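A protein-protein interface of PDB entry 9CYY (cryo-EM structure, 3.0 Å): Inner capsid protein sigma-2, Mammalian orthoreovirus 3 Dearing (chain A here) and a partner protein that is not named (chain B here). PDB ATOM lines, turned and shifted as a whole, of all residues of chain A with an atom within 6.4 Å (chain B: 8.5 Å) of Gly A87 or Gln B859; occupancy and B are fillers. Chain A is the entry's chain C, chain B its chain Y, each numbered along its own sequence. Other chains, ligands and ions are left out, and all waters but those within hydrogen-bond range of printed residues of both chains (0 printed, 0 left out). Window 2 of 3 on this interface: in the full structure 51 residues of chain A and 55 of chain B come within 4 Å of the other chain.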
ATOM      1  N   ILE A  78     -18.621 -10.381 -24.535  1.00  0.00           N
ATOM      2  CA  ILE A  78     -17.919 -11.656 -24.694  1.00  0.00           C
ATOM      3  C   ILE A  78     -18.368 -12.404 -25.945  1.00  0.00           C
ATOM      4  O   ILE A  78     -17.512 -12.724 -26.785  1.00  0.00           O
ATOM      5  CB  ILE A  78     -18.050 -12.499 -23.414  1.00  0.00           C
ATOM      6  CG1 ILE A  78     -17.282 -11.851 -22.264  1.00  0.00           C
ATOM      7  CG2 ILE A  78     -17.562 -13.911 -23.659  1.00  0.00           C
ATOM      8  CD1 ILE A  78     -17.655 -12.394 -20.908  1.00  0.00           C
ATOM      9  N   ARG A  81     -17.431 -10.796 -29.674  1.00  0.00           N
ATOM     10  CA  ARG A  81     -16.112 -10.728 -30.269  1.00  0.00           C
ATOM     11  C   ARG A  81     -16.137 -11.407 -31.635  1.00  0.00           C
ATOM     12  O   ARG A  81     -17.006 -12.238 -31.905  1.00  0.00           O
ATOM     13  CB  ARG A  81     -15.086 -11.396 -29.358  1.00  0.00           C
ATOM     14  CG  ARG A  81     -14.820 -10.644 -28.072  1.00  0.00           C
ATOM     15  CD  ARG A  81     -14.046 -11.499 -27.087  1.00  0.00           C
ATOM     16  NE  ARG A  81     -14.644 -12.818 -26.922  1.00  0.00           N
ATOM     17  CZ  ARG A  81     -13.971 -13.905 -26.570  1.00  0.00           C
ATOM     18  NH1 ARG A  81     -12.669 -13.867 -26.343  1.00  0.00           N
ATOM     19  NH2 ARG A  81     -14.621 -15.056 -26.440  1.00  0.00           N
ATOM     20  N   ARG A  85     -16.897 -16.824 -29.635  1.00  0.00           N
ATOM     21  CA  ARG A  85     -16.937 -17.809 -28.563  1.00  0.00           C
ATOM     22  C   ARG A  85     -17.679 -17.244 -27.359  1.00  0.00           C
ATOM     23  O   ARG A  85     -17.570 -16.058 -27.043  1.00  0.00           O
ATOM     24  CB  ARG A  85     -15.526 -18.231 -28.165  1.00  0.00           C
ATOM     25  CG  ARG A  85     -14.792 -19.019 -29.229  1.00  0.00           C
ATOM     26  CD  ARG A  85     -13.403 -19.398 -28.755  1.00  0.00           C
ATOM     27  NE  ARG A  85     -12.685 -20.180 -29.753  1.00  0.00           N
ATOM     28  CZ  ARG A  85     -11.906 -19.662 -30.692  1.00  0.00           C
ATOM     29  NH1 ARG A  85     -11.700 -18.359 -30.776  1.00  0.00           N
ATOM     30  NH2 ARG A  85     -11.318 -20.473 -31.566  1.00  0.00           N
ATOM     31  N   TRP A  86     -18.437 -18.104 -26.681  1.00  0.00           N
ATOM     32  CA  TRP A  86     -19.337 -17.665 -25.621  1.00  0.00           C
ATOM     33  C   TRP A  86     -18.834 -17.978 -24.218  1.00  0.00           C
ATOM     34  O   TRP A  86     -19.122 -17.222 -23.287  1.00  0.00           O
ATOM     35  CB  TRP A  86     -20.719 -18.296 -25.810  1.00  0.00           C
ATOM     36  CG  TRP A  86     -20.700 -19.790 -25.822  1.00  0.00           C
ATOM     37  CD1 TRP A  86     -20.528 -20.596 -26.906  1.00  0.00           C
ATOM     38  CD2 TRP A  86     -20.862 -20.661 -24.697  1.00  0.00           C
ATOM     39  NE1 TRP A  86     -20.569 -21.915 -26.527  1.00  0.00           N
ATOM     40  CE2 TRP A  86     -20.773 -21.981 -25.175  1.00  0.00           C
ATOM     41  CE3 TRP A  86     -21.072 -20.452 -23.332  1.00  0.00           C
ATOM     42  CZ2 TRP A  86     -20.886 -23.086 -24.337  1.00  0.00           C
ATOM     43  CZ3 TRP A  86     -21.183 -21.550 -22.502  1.00  0.00           C
ATOM     44  CH2 TRP A  86     -21.090 -22.850 -23.008  1.00  0.00           C
ATOM     45  N   GLY A  87     -18.095 -19.067 -24.032  1.00  0.00           N
ATOM     46  CA  GLY A  87     -17.771 -19.494 -22.684  1.00  0.00           C
ATOM     47  C   GLY A  87     -16.317 -19.806 -22.402  1.00  0.00           C
ATOM     48  O   GLY A  87     -16.021 -20.739 -21.651  1.00  0.00           O
ATOM     49  N   ASP A  88     -15.395 -19.038 -22.983  1.00  0.00           N
ATOM     50  CA  ASP A  88     -13.974 -19.256 -22.760  1.00  0.00           C
ATOM     51  C   ASP A  88     -13.298 -18.163 -21.948  1.00  0.00           C
ATOM     52  O   ASP A  88     -12.176 -18.378 -21.480  1.00  0.00           O
ATOM     53  CB  ASP A  88     -13.236 -19.398 -24.100  1.00  0.00           C
ATOM     54  CG  ASP A  88     -13.505 -18.242 -25.034  1.00  0.00           C
ATOM     55  OD1 ASP A  88     -14.678 -17.833 -25.148  1.00  0.00           O
ATOM     56  OD2 ASP A  88     -12.545 -17.744 -25.657  1.00  0.00           O
ATOM     57  N   ILE A  89     -13.935 -17.009 -21.766  1.00  0.00           N
ATOM     58  CA  ILE A  89     -13.359 -15.899 -21.023  1.00  0.00           C
ATOM     59  C   ILE A  89     -14.377 -15.441 -19.983  1.00  0.00           C
ATOM     60  O   ILE A  89     -15.572 -15.714 -20.088  1.00  0.00           O
ATOM     61  CB  ILE A  89     -12.939 -14.738 -21.946  1.00  0.00           C
ATOM     62  CG1 ILE A  89     -11.889 -13.856 -21.269  1.00  0.00           C
ATOM     63  CG2 ILE A  89     -14.142 -13.913 -22.351  1.00  0.00           C
ATOM     64  CD1 ILE A  89     -10.570 -14.549 -21.047  1.00  0.00           C
ATOM     65  N   VAL A  95     -19.328 -16.087 -15.964  1.00  0.00           N
ATOM     66  CA  VAL A  95     -19.274 -16.708 -17.278  1.00  0.00           C
ATOM     67  C   VAL A  95     -20.686 -17.049 -17.725  1.00  0.00           C
ATOM     68  O   VAL A  95     -21.564 -17.358 -16.912  1.00  0.00           O
ATOM     69  CB  VAL A  95     -18.387 -17.972 -17.292  1.00  0.00           C
ATOM     70  CG1 VAL A  95     -16.920 -17.593 -17.221  1.00  0.00           C
ATOM     71  CG2 VAL A  95     -18.759 -18.891 -16.148  1.00  0.00           C
ATOM     72  N   TRP A  96     -20.900 -16.986 -19.035  1.00  0.00           N
ATOM     73  CA  TRP A  96     -22.180 -17.367 -19.611  1.00  0.00           C
ATOM     74  C   TRP A  96     -22.401 -18.866 -19.476  1.00  0.00           C
ATOM     75  O   TRP A  96     -21.457 -19.658 -19.537  1.00  0.00           O
ATOM     76  CB  TRP A  96     -22.238 -16.972 -21.084  1.00  0.00           C
ATOM     77  CG  TRP A  96     -22.487 -15.523 -21.319  1.00  0.00           C
ATOM     78  CD1 TRP A  96     -21.577 -14.591 -21.717  1.00  0.00           C
ATOM     79  CD2 TRP A  96     -23.734 -14.836 -21.186  1.00  0.00           C
ATOM     80  NE1 TRP A  96     -22.179 -13.364 -21.833  1.00  0.00           N
ATOM     81  CE2 TRP A  96     -23.504 -13.488 -21.511  1.00  0.00           C
ATOM     82  CE3 TRP A  96     -25.021 -15.231 -20.818  1.00  0.00           C
ATOM     83  CZ2 TRP A  96     -24.514 -12.534 -21.484  1.00  0.00           C
ATOM     84  CZ3 TRP A  96     -26.021 -14.282 -20.788  1.00  0.00           C
ATOM     85  CH2 TRP A  96     -25.763 -12.950 -21.119  1.00  0.00           C
ATOM     86  N   SER A  97     -23.657 -19.256 -19.293  1.00  0.00           N
ATOM     87  CA  SER A  97     -24.062 -20.655 -19.316  1.00  0.00           C
ATOM     88  C   SER A  97     -24.893 -20.867 -20.574  1.00  0.00           C
ATOM     89  O   SER A  97     -25.902 -20.183 -20.774  1.00  0.00           O
ATOM     90  CB  SER A  97     -24.852 -21.020 -18.063  1.00  0.00           C
ATOM     91  OG  SER A  97     -25.973 -20.171 -17.908  1.00  0.00           O
ATOM     92  N   ALA A  98     -24.441 -21.786 -21.432  1.00  0.00           N
ATOM     93  CA  ALA A  98     -25.085 -22.176 -22.685  1.00  0.00           C
ATOM     94  C   ALA A  98     -24.913 -21.090 -23.740  1.00  0.00           C
ATOM     95  O   ALA A  98     -24.897 -19.897 -23.413  1.00  0.00           O
ATOM     96  CB  ALA A  98     -26.568 -22.493 -22.478  1.00  0.00           C
ATOM     97  N   VAL A 105     -22.950 -17.614 -14.348  1.00  0.00           N
ATOM     98  CA  VAL A 105     -22.516 -18.459 -13.244  1.00  0.00           C
ATOM     99  C   VAL A 105     -21.073 -18.123 -12.896  1.00  0.00           C
ATOM    100  O   VAL A 105     -20.383 -17.407 -13.621  1.00  0.00           O
ATOM    101  CB  VAL A 105     -22.656 -19.961 -13.568  1.00  0.00           C
ATOM    102  CG1 VAL A 105     -24.115 -20.330 -13.747  1.00  0.00           C
ATOM    103  CG2 VAL A 105     -21.877 -20.298 -14.820  1.00  0.00           C
ATOM    104  N   VAL A 106     -20.629 -18.639 -11.748  1.00  0.00           N
ATOM    105  CA  VAL A 106     -19.253 -18.415 -11.328  1.00  0.00           C
ATOM    106  C   VAL A 106     -18.307 -19.145 -12.276  1.00  0.00           C
ATOM    107  O   VAL A 106     -18.614 -20.229 -12.788  1.00  0.00           O
ATOM    108  CB  VAL A 106     -19.045 -18.872  -9.875  1.00  0.00           C
ATOM    109  CG1 VAL A 106     -17.723 -18.358  -9.337  1.00  0.00           C
ATOM    110  CG2 VAL A 106     -20.193 -18.395  -9.007  1.00  0.00           C
ATOM    111  N   ALA A 107     -17.147 -18.545 -12.516  1.00  0.00           N
ATOM    112  CA  ALA A 107     -16.208 -19.104 -13.471  1.00  0.00           C
ATOM    113  C   ALA A 107     -15.586 -20.394 -12.935  1.00  0.00           C
ATOM    114  O   ALA A 107     -15.443 -20.568 -11.723  1.00  0.00           O
ATOM    115  CB  ALA A 107     -15.109 -18.097 -13.789  1.00  0.00           C
ATOM    116  N   PRO A 108     -15.218 -21.315 -13.821  1.00  0.00           N
ATOM    117  CA  PRO A 108     -14.479 -22.508 -13.400  1.00  0.00           C
ATOM    118  C   PRO A 108     -13.093 -22.136 -12.907  1.00  0.00           C
ATOM    119  O   PRO A 108     -12.634 -21.005 -13.129  1.00  0.00           O
ATOM    120  CB  PRO A 108     -14.411 -23.349 -14.684  1.00  0.00           C
ATOM    121  CG  PRO A 108     -15.530 -22.847 -15.526  1.00  0.00           C
ATOM    122  CD  PRO A 108     -15.611 -21.385 -15.237  1.00  0.00           C
ATOM    123  N   VAL A 111     -10.646 -20.759 -15.690  1.00  0.00           N
ATOM    124  CA  VAL A 111     -10.992 -19.425 -16.164  1.00  0.00           C
ATOM    125  C   VAL A 111     -10.724 -18.390 -15.083  1.00  0.00           C
ATOM    126  O   VAL A 111     -10.326 -17.258 -15.380  1.00  0.00           O
ATOM    127  CB  VAL A 111     -12.457 -19.396 -16.635  1.00  0.00           C
ATOM    128  CG1 VAL A 111     -12.785 -18.057 -17.254  1.00  0.00           C
ATOM    129  CG2 VAL A 111     -12.712 -20.518 -17.624  1.00  0.00           C
ATOM    130  N   GLN B 852     -28.270 -32.422 -11.850  1.00  0.00           N
ATOM    131  CA  GLN B 852     -27.069 -32.217 -11.053  1.00  0.00           C
ATOM    132  C   GLN B 852     -25.952 -31.704 -11.947  1.00  0.00           C
ATOM    133  O   GLN B 852     -26.165 -31.356 -13.110  1.00  0.00           O
ATOM    134  CB  GLN B 852     -26.629 -33.502 -10.344  1.00  0.00           C
ATOM    135  CG  GLN B 852     -27.600 -34.011  -9.300  1.00  0.00           C
ATOM    136  CD  GLN B 852     -27.452 -35.497  -9.049  1.00  0.00           C
ATOM    137  OE1 GLN B 852     -26.841 -35.915  -8.067  1.00  0.00           O
ATOM    138  NE2 GLN B 852     -28.014 -36.305  -9.940  1.00  0.00           N
ATOM    139  N   SER B 853     -24.748 -31.663 -11.385  1.00  0.00           N
ATOM    140  CA  SER B 853     -23.549 -31.238 -12.089  1.00  0.00           C
ATOM    141  C   SER B 853     -22.368 -32.100 -11.656  1.00  0.00           C
ATOM    142  O   SER B 853     -22.388 -32.744 -10.604  1.00  0.00           O
ATOM    143  CB  SER B 853     -23.260 -29.755 -11.835  1.00  0.00           C
ATOM    144  OG  SER B 853     -22.108 -29.337 -12.543  1.00  0.00           O
ATOM    145  N   ARG B 854     -21.332 -32.103 -12.482  1.00  0.00           N
ATOM    146  CA  ARG B 854     -20.181 -32.982 -12.321  1.00  0.00           C
ATOM    147  C   ARG B 854     -19.121 -32.265 -11.477  1.00  0.00           C
ATOM    148  O   ARG B 854     -19.474 -31.291 -10.806  1.00  0.00           O
ATOM    149  CB  ARG B 854     -19.704 -33.473 -13.685  1.00  0.00           C
ATOM    150  CG  ARG B 854     -20.442 -34.699 -14.170  1.00  0.00           C
ATOM    151  CD  ARG B 854     -19.856 -35.215 -15.465  1.00  0.00           C
ATOM    152  NE  ARG B 854     -18.445 -35.545 -15.318  1.00  0.00           N
ATOM    153  CZ  ARG B 854     -17.460 -34.907 -15.933  1.00  0.00           C
ATOM    154  NH1 ARG B 854     -17.697 -33.902 -16.759  1.00  0.00           N
ATOM    155  NH2 ARG B 854     -16.205 -35.286 -15.712  1.00  0.00           N
ATOM    156  N   THR B 856     -16.224 -30.172 -11.279  1.00  0.00           N
ATOM    157  CA  THR B 856     -16.051 -28.729 -11.237  1.00  0.00           C
ATOM    158  C   THR B 856     -16.742 -28.039 -12.402  1.00  0.00           C
ATOM    159  O   THR B 856     -16.582 -26.827 -12.579  1.00  0.00           O
ATOM    160  CB  THR B 856     -14.565 -28.367 -11.224  1.00  0.00           C
ATOM    161  OG1 THR B 856     -13.906 -29.012 -12.319  1.00  0.00           O
ATOM    162  CG2 THR B 856     -13.922 -28.805  -9.921  1.00  0.00           C
ATOM    163  N   ILE B 857     -17.501 -28.784 -13.205  1.00  0.00           N
ATOM    164  CA  ILE B 857     -18.214 -28.189 -14.323  1.00  0.00           C
ATOM    165  C   ILE B 857     -19.306 -27.276 -13.789  1.00  0.00           C
ATOM    166  O   ILE B 857     -20.152 -27.694 -12.989  1.00  0.00           O
ATOM    167  CB  ILE B 857     -18.793 -29.279 -15.235  1.00  0.00           C
ATOM    168  CG1 ILE B 857     -17.706 -30.282 -15.616  1.00  0.00           C
ATOM    169  CG2 ILE B 857     -19.391 -28.658 -16.481  1.00  0.00           C
ATOM    170  CD1 ILE B 857     -16.539 -29.664 -16.343  1.00  0.00           C
ATOM    171  N   THR B 858     -19.290 -26.020 -14.227  1.00  0.00           N
ATOM    172  CA  THR B 858     -20.243 -25.027 -13.763  1.00  0.00           C
ATOM    173  C   THR B 858     -21.307 -24.684 -14.794  1.00  0.00           C
ATOM    174  O   THR B 858     -22.425 -24.330 -14.412  1.00  0.00           O
ATOM    175  CB  THR B 858     -19.503 -23.745 -13.354  1.00  0.00           C
ATOM    176  OG1 THR B 858     -18.443 -24.077 -12.450  1.00  0.00           O
ATOM    177  CG2 THR B 858     -20.435 -22.785 -12.666  1.00  0.00           C
ATOM    178  N   GLN B 859     -20.998 -24.809 -16.079  1.00  0.00           N
ATOM    179  CA  GLN B 859     -21.923 -24.427 -17.133  1.00  0.00           C
ATOM    180  C   GLN B 859     -22.739 -25.637 -17.563  1.00  0.00           C
ATOM    181  O   GLN B 859     -22.155 -26.660 -17.939  1.00  0.00           O
ATOM    182  CB  GLN B 859     -21.163 -23.853 -18.312  1.00  0.00           C
ATOM    183  CG  GLN B 859     -20.314 -22.652 -17.926  1.00  0.00           C
ATOM    184  CD  GLN B 859     -19.360 -22.229 -19.016  1.00  0.00           C
ATOM    185  OE1 GLN B 859     -19.267 -22.872 -20.060  1.00  0.00           O
ATOM    186  NE2 GLN B 859     -18.637 -21.143 -18.778  1.00  0.00           N
ATOM    187  N   PRO B 860     -24.073 -25.572 -17.516  1.00  0.00           N
ATOM    188  CA  PRO B 860     -24.881 -26.755 -17.855  1.00  0.00           C
ATOM    189  C   PRO B 860     -24.650 -27.275 -19.261  1.00  0.00           C
ATOM    190  O   PRO B 860     -24.826 -28.475 -19.504  1.00  0.00           O
ATOM    191  CB  PRO B 860     -26.319 -26.252 -17.675  1.00  0.00           C
ATOM    192  CG  PRO B 860     -26.202 -25.117 -16.723  1.00  0.00           C
ATOM    193  CD  PRO B 860     -24.903 -24.453 -17.049  1.00  0.00           C
ATOM    194  N   ALA B 861     -24.284 -26.406 -20.203  1.00  0.00           N
ATOM    195  CA  ALA B 861     -24.044 -26.854 -21.569  1.00  0.00           C
ATOM    196  C   ALA B 861     -22.847 -27.788 -21.672  1.00  0.00           C
ATOM    197  O   ALA B 861     -22.699 -28.473 -22.688  1.00  0.00           O
ATOM    198  CB  ALA B 861     -23.847 -25.653 -22.490  1.00  0.00           C
ATOM    199  N   LEU B 862     -21.993 -27.830 -20.654  1.00  0.00           N
ATOM    200  CA  LEU B 862     -20.813 -28.683 -20.667  1.00  0.00           C
ATOM    201  C   LEU B 862     -20.996 -29.969 -19.873  1.00  0.00           C
ATOM    202  O   LEU B 862     -20.170 -30.878 -20.001  1.00  0.00           O
ATOM    203  CB  LEU B 862     -19.605 -27.912 -20.128  1.00  0.00           C
ATOM    204  CG  LEU B 862     -19.338 -26.551 -20.771  1.00  0.00           C
ATOM    205  CD1 LEU B 862     -18.039 -25.963 -20.253  1.00  0.00           C
ATOM    206  CD2 LEU B 862     -19.304 -26.672 -22.283  1.00  0.00           C
ATOM    207  N   SER B 863     -22.048 -30.074 -19.063  1.00  0.00           N
ATOM    208  CA  SER B 863     -22.294 -31.267 -18.269  1.00  0.00           C
ATOM    209  C   SER B 863     -23.607 -31.962 -18.592  1.00  0.00           C
ATOM    210  O   SER B 863     -23.861 -33.046 -18.051  1.00  0.00           O
ATOM    211  CB  SER B 863     -22.268 -30.926 -16.771  1.00  0.00           C
ATOM    212  OG  SER B 863     -23.372 -30.113 -16.418  1.00  0.00           O
ATOM    213  N   LEU B 864     -24.453 -31.369 -19.437  1.00  0.00           N
ATOM    214  CA  LEU B 864     -25.706 -32.017 -19.807  1.00  0.00           C
ATOM    215  C   LEU B 864     -25.458 -33.320 -20.552  1.00  0.00           C
ATOM    216  O   LEU B 864     -26.233 -34.275 -20.423  1.00  0.00           O
ATOM    217  CB  LEU B 864     -26.546 -31.062 -20.657  1.00  0.00           C
ATOM    218  CG  LEU B 864     -27.889 -31.554 -21.191  1.00  0.00           C
ATOM    219  CD1 LEU B 864     -28.712 -32.197 -20.094  1.00  0.00           C
ATOM    220  CD2 LEU B 864     -28.646 -30.404 -21.820  1.00  0.00           C
ATOM    221  N   SER B 865     -24.380 -33.381 -21.333  1.00  0.00           N
ATOM    222  CA  SER B 865     -24.128 -34.559 -22.156  1.00  0.00           C
ATOM    223  C   SER B 865     -23.863 -35.792 -21.301  1.00  0.00           C
ATOM    224  O   SER B 865     -24.220 -36.911 -21.689  1.00  0.00           O
ATOM    225  CB  SER B 865     -22.953 -34.297 -23.095  1.00  0.00           C
ATOM    226  OG  SER B 865     -21.741 -34.197 -22.371  1.00  0.00           O
ATOM    227  N   THR B 867     -24.426 -35.908 -17.662  1.00  0.00           N
ATOM    228  CA  THR B 867     -25.109 -35.943 -16.373  1.00  0.00           C
ATOM    229  C   THR B 867     -26.624 -35.996 -16.600  1.00  0.00           C
ATOM    230  O   THR B 867     -27.406 -35.241 -16.035  1.00  0.00           O
ATOM    231  CB  THR B 867     -24.694 -34.742 -15.524  1.00  0.00           C
ATOM    232  OG1 THR B 867     -23.267 -34.688 -15.464  1.00  0.00           O
ATOM    233  CG2 THR B 867     -25.198 -34.885 -14.096  1.00  0.00           C
ATOM    234  N   GLN B 942     -22.611 -22.970  -7.309  1.00  0.00           N
ATOM    235  CA  GLN B 942     -22.113 -22.322  -8.510  1.00  0.00           C
ATOM    236  C   GLN B 942     -22.878 -21.058  -8.876  1.00  0.00           C
ATOM    237  O   GLN B 942     -22.588 -20.459  -9.916  1.00  0.00           O
ATOM    238  CB  GLN B 942     -22.155 -23.298  -9.687  1.00  0.00           C
ATOM    239  CG  GLN B 942     -23.542 -23.554 -10.242  1.00  0.00           C
ATOM    240  CD  GLN B 942     -24.216 -24.743  -9.597  1.00  0.00           C
ATOM    241  OE1 GLN B 942     -23.803 -25.202  -8.535  1.00  0.00           O
ATOM    242  NE2 GLN B 942     -25.259 -25.251 -10.239  1.00  0.00           N
ATOM    243  N   GLN B 996     -29.460 -28.016 -11.230  1.00  0.00           N
ATOM    244  CA  GLN B 996     -29.659 -27.403 -12.535  1.00  0.00           C
ATOM    245  C   GLN B 996     -30.768 -28.163 -13.243  1.00  0.00           C
ATOM    246  O   GLN B 996     -31.145 -29.261 -12.829  1.00  0.00           O
ATOM    247  CB  GLN B 996     -28.371 -27.410 -13.363  1.00  0.00           C
ATOM    248  CG  GLN B 996     -28.073 -28.733 -14.034  1.00  0.00           C
ATOM    249  CD  GLN B 996     -26.683 -28.778 -14.626  1.00  0.00           C
ATOM    250  OE1 GLN B 996     -25.863 -27.894 -14.381  1.00  0.00           O
ATOM    251  NE2 GLN B 996     -26.404 -29.814 -15.405  1.00  0.00           N
ATOM    252  N   ILE B1012     -32.043 -25.283 -22.367  1.00  0.00           N
ATOM    253  CA  ILE B1012     -31.726 -24.840 -21.012  1.00  0.00           C
ATOM    254  C   ILE B1012     -32.647 -23.676 -20.668  1.00  0.00           C
ATOM    255  O   ILE B1012     -32.422 -22.551 -21.137  1.00  0.00           O
ATOM    256  CB  ILE B1012     -30.247 -24.443 -20.876  1.00  0.00           C
ATOM    257  CG1 ILE B1012     -29.344 -25.660 -21.072  1.00  0.00           C
ATOM    258  CG2 ILE B1012     -29.988 -23.823 -19.516  1.00  0.00           C
ATOM    259  CD1 ILE B1012     -28.816 -25.811 -22.477  1.00  0.00           C
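Of the printed residues of chain B, Trp A86 touches Gln B859 (3.4 Å) and Ala B861 (3.97 Å). Printed residues of chain B within 4 Å of Val A106: Thr B858 and Gln B942. Of chain A, only Trp A86, Gly A87, Val A95 and Trp A96 come within 4 Å of Gln B859. Of the printed residues of chain A, Pro B860 touches Ser A97. Printed residues of chain A within 4 Å of Ala B861: Trp A86 and Ala A98. The nearest residue of chain B that does not touch Gly A87 is Leu B862 (5.8 Å).
Of the 17 printed residues of chain B, 5 touch a printed residue of chain A. Along chain B the printed residues that touch a printed residue of chain A span positions 858 to 942. Of the 16 printed residues of chain A, 8 touch a printed residue of chain B. Hydrophobic or aromatic side chains of chain A within 4 Å of the printed part of chain B: Trp A86, Val A95, Val A105 and Val A106. Among the printed residues, no Asp or Glu carboxylate lies within 4 Å of a Lys or Arg side-chain nitrogen of the other chain.
The backbone carbonyl oxygen (O) of Val A105 sits at hydrogen-bond distance from the backbone NH (N) of Val A95, 2.9 Å away. The side-chain hydroxyl of Thr B858 lies within hydrogen-bond range of the backbone carbonyl oxygen of Thr B856, at 3.3 Å.
The backbone carbonyl oxygen (O) of Trp A96 is in hydrogen-bond range of the side-chain amide nitrogen (NE2) of Gln B859 (3.3 Å). The backbone carbonyl oxygen of Gln B942 is in hydrogen-bond range of the backbone NH of Val A106 (3.2 Å).
Among the printed residues, merely in contact across the chains: Trp A86 with Gln B859 (3.4 Å), Trp A86 with Ala B861 (3.97 Å), Gly A87 with Gln B859 (3.9 Å), Val A95 with Gln B859 (3.5 Å), Ser A97 with Pro B860 (3.6 Å), Ala A98 with Ala B861 (3.7 Å), Val A105 with Thr B858 (3.6 Å), Val A105 with Gln B942 (3.7 Å) and Val A106 with Thr B858 (3.1 Å).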
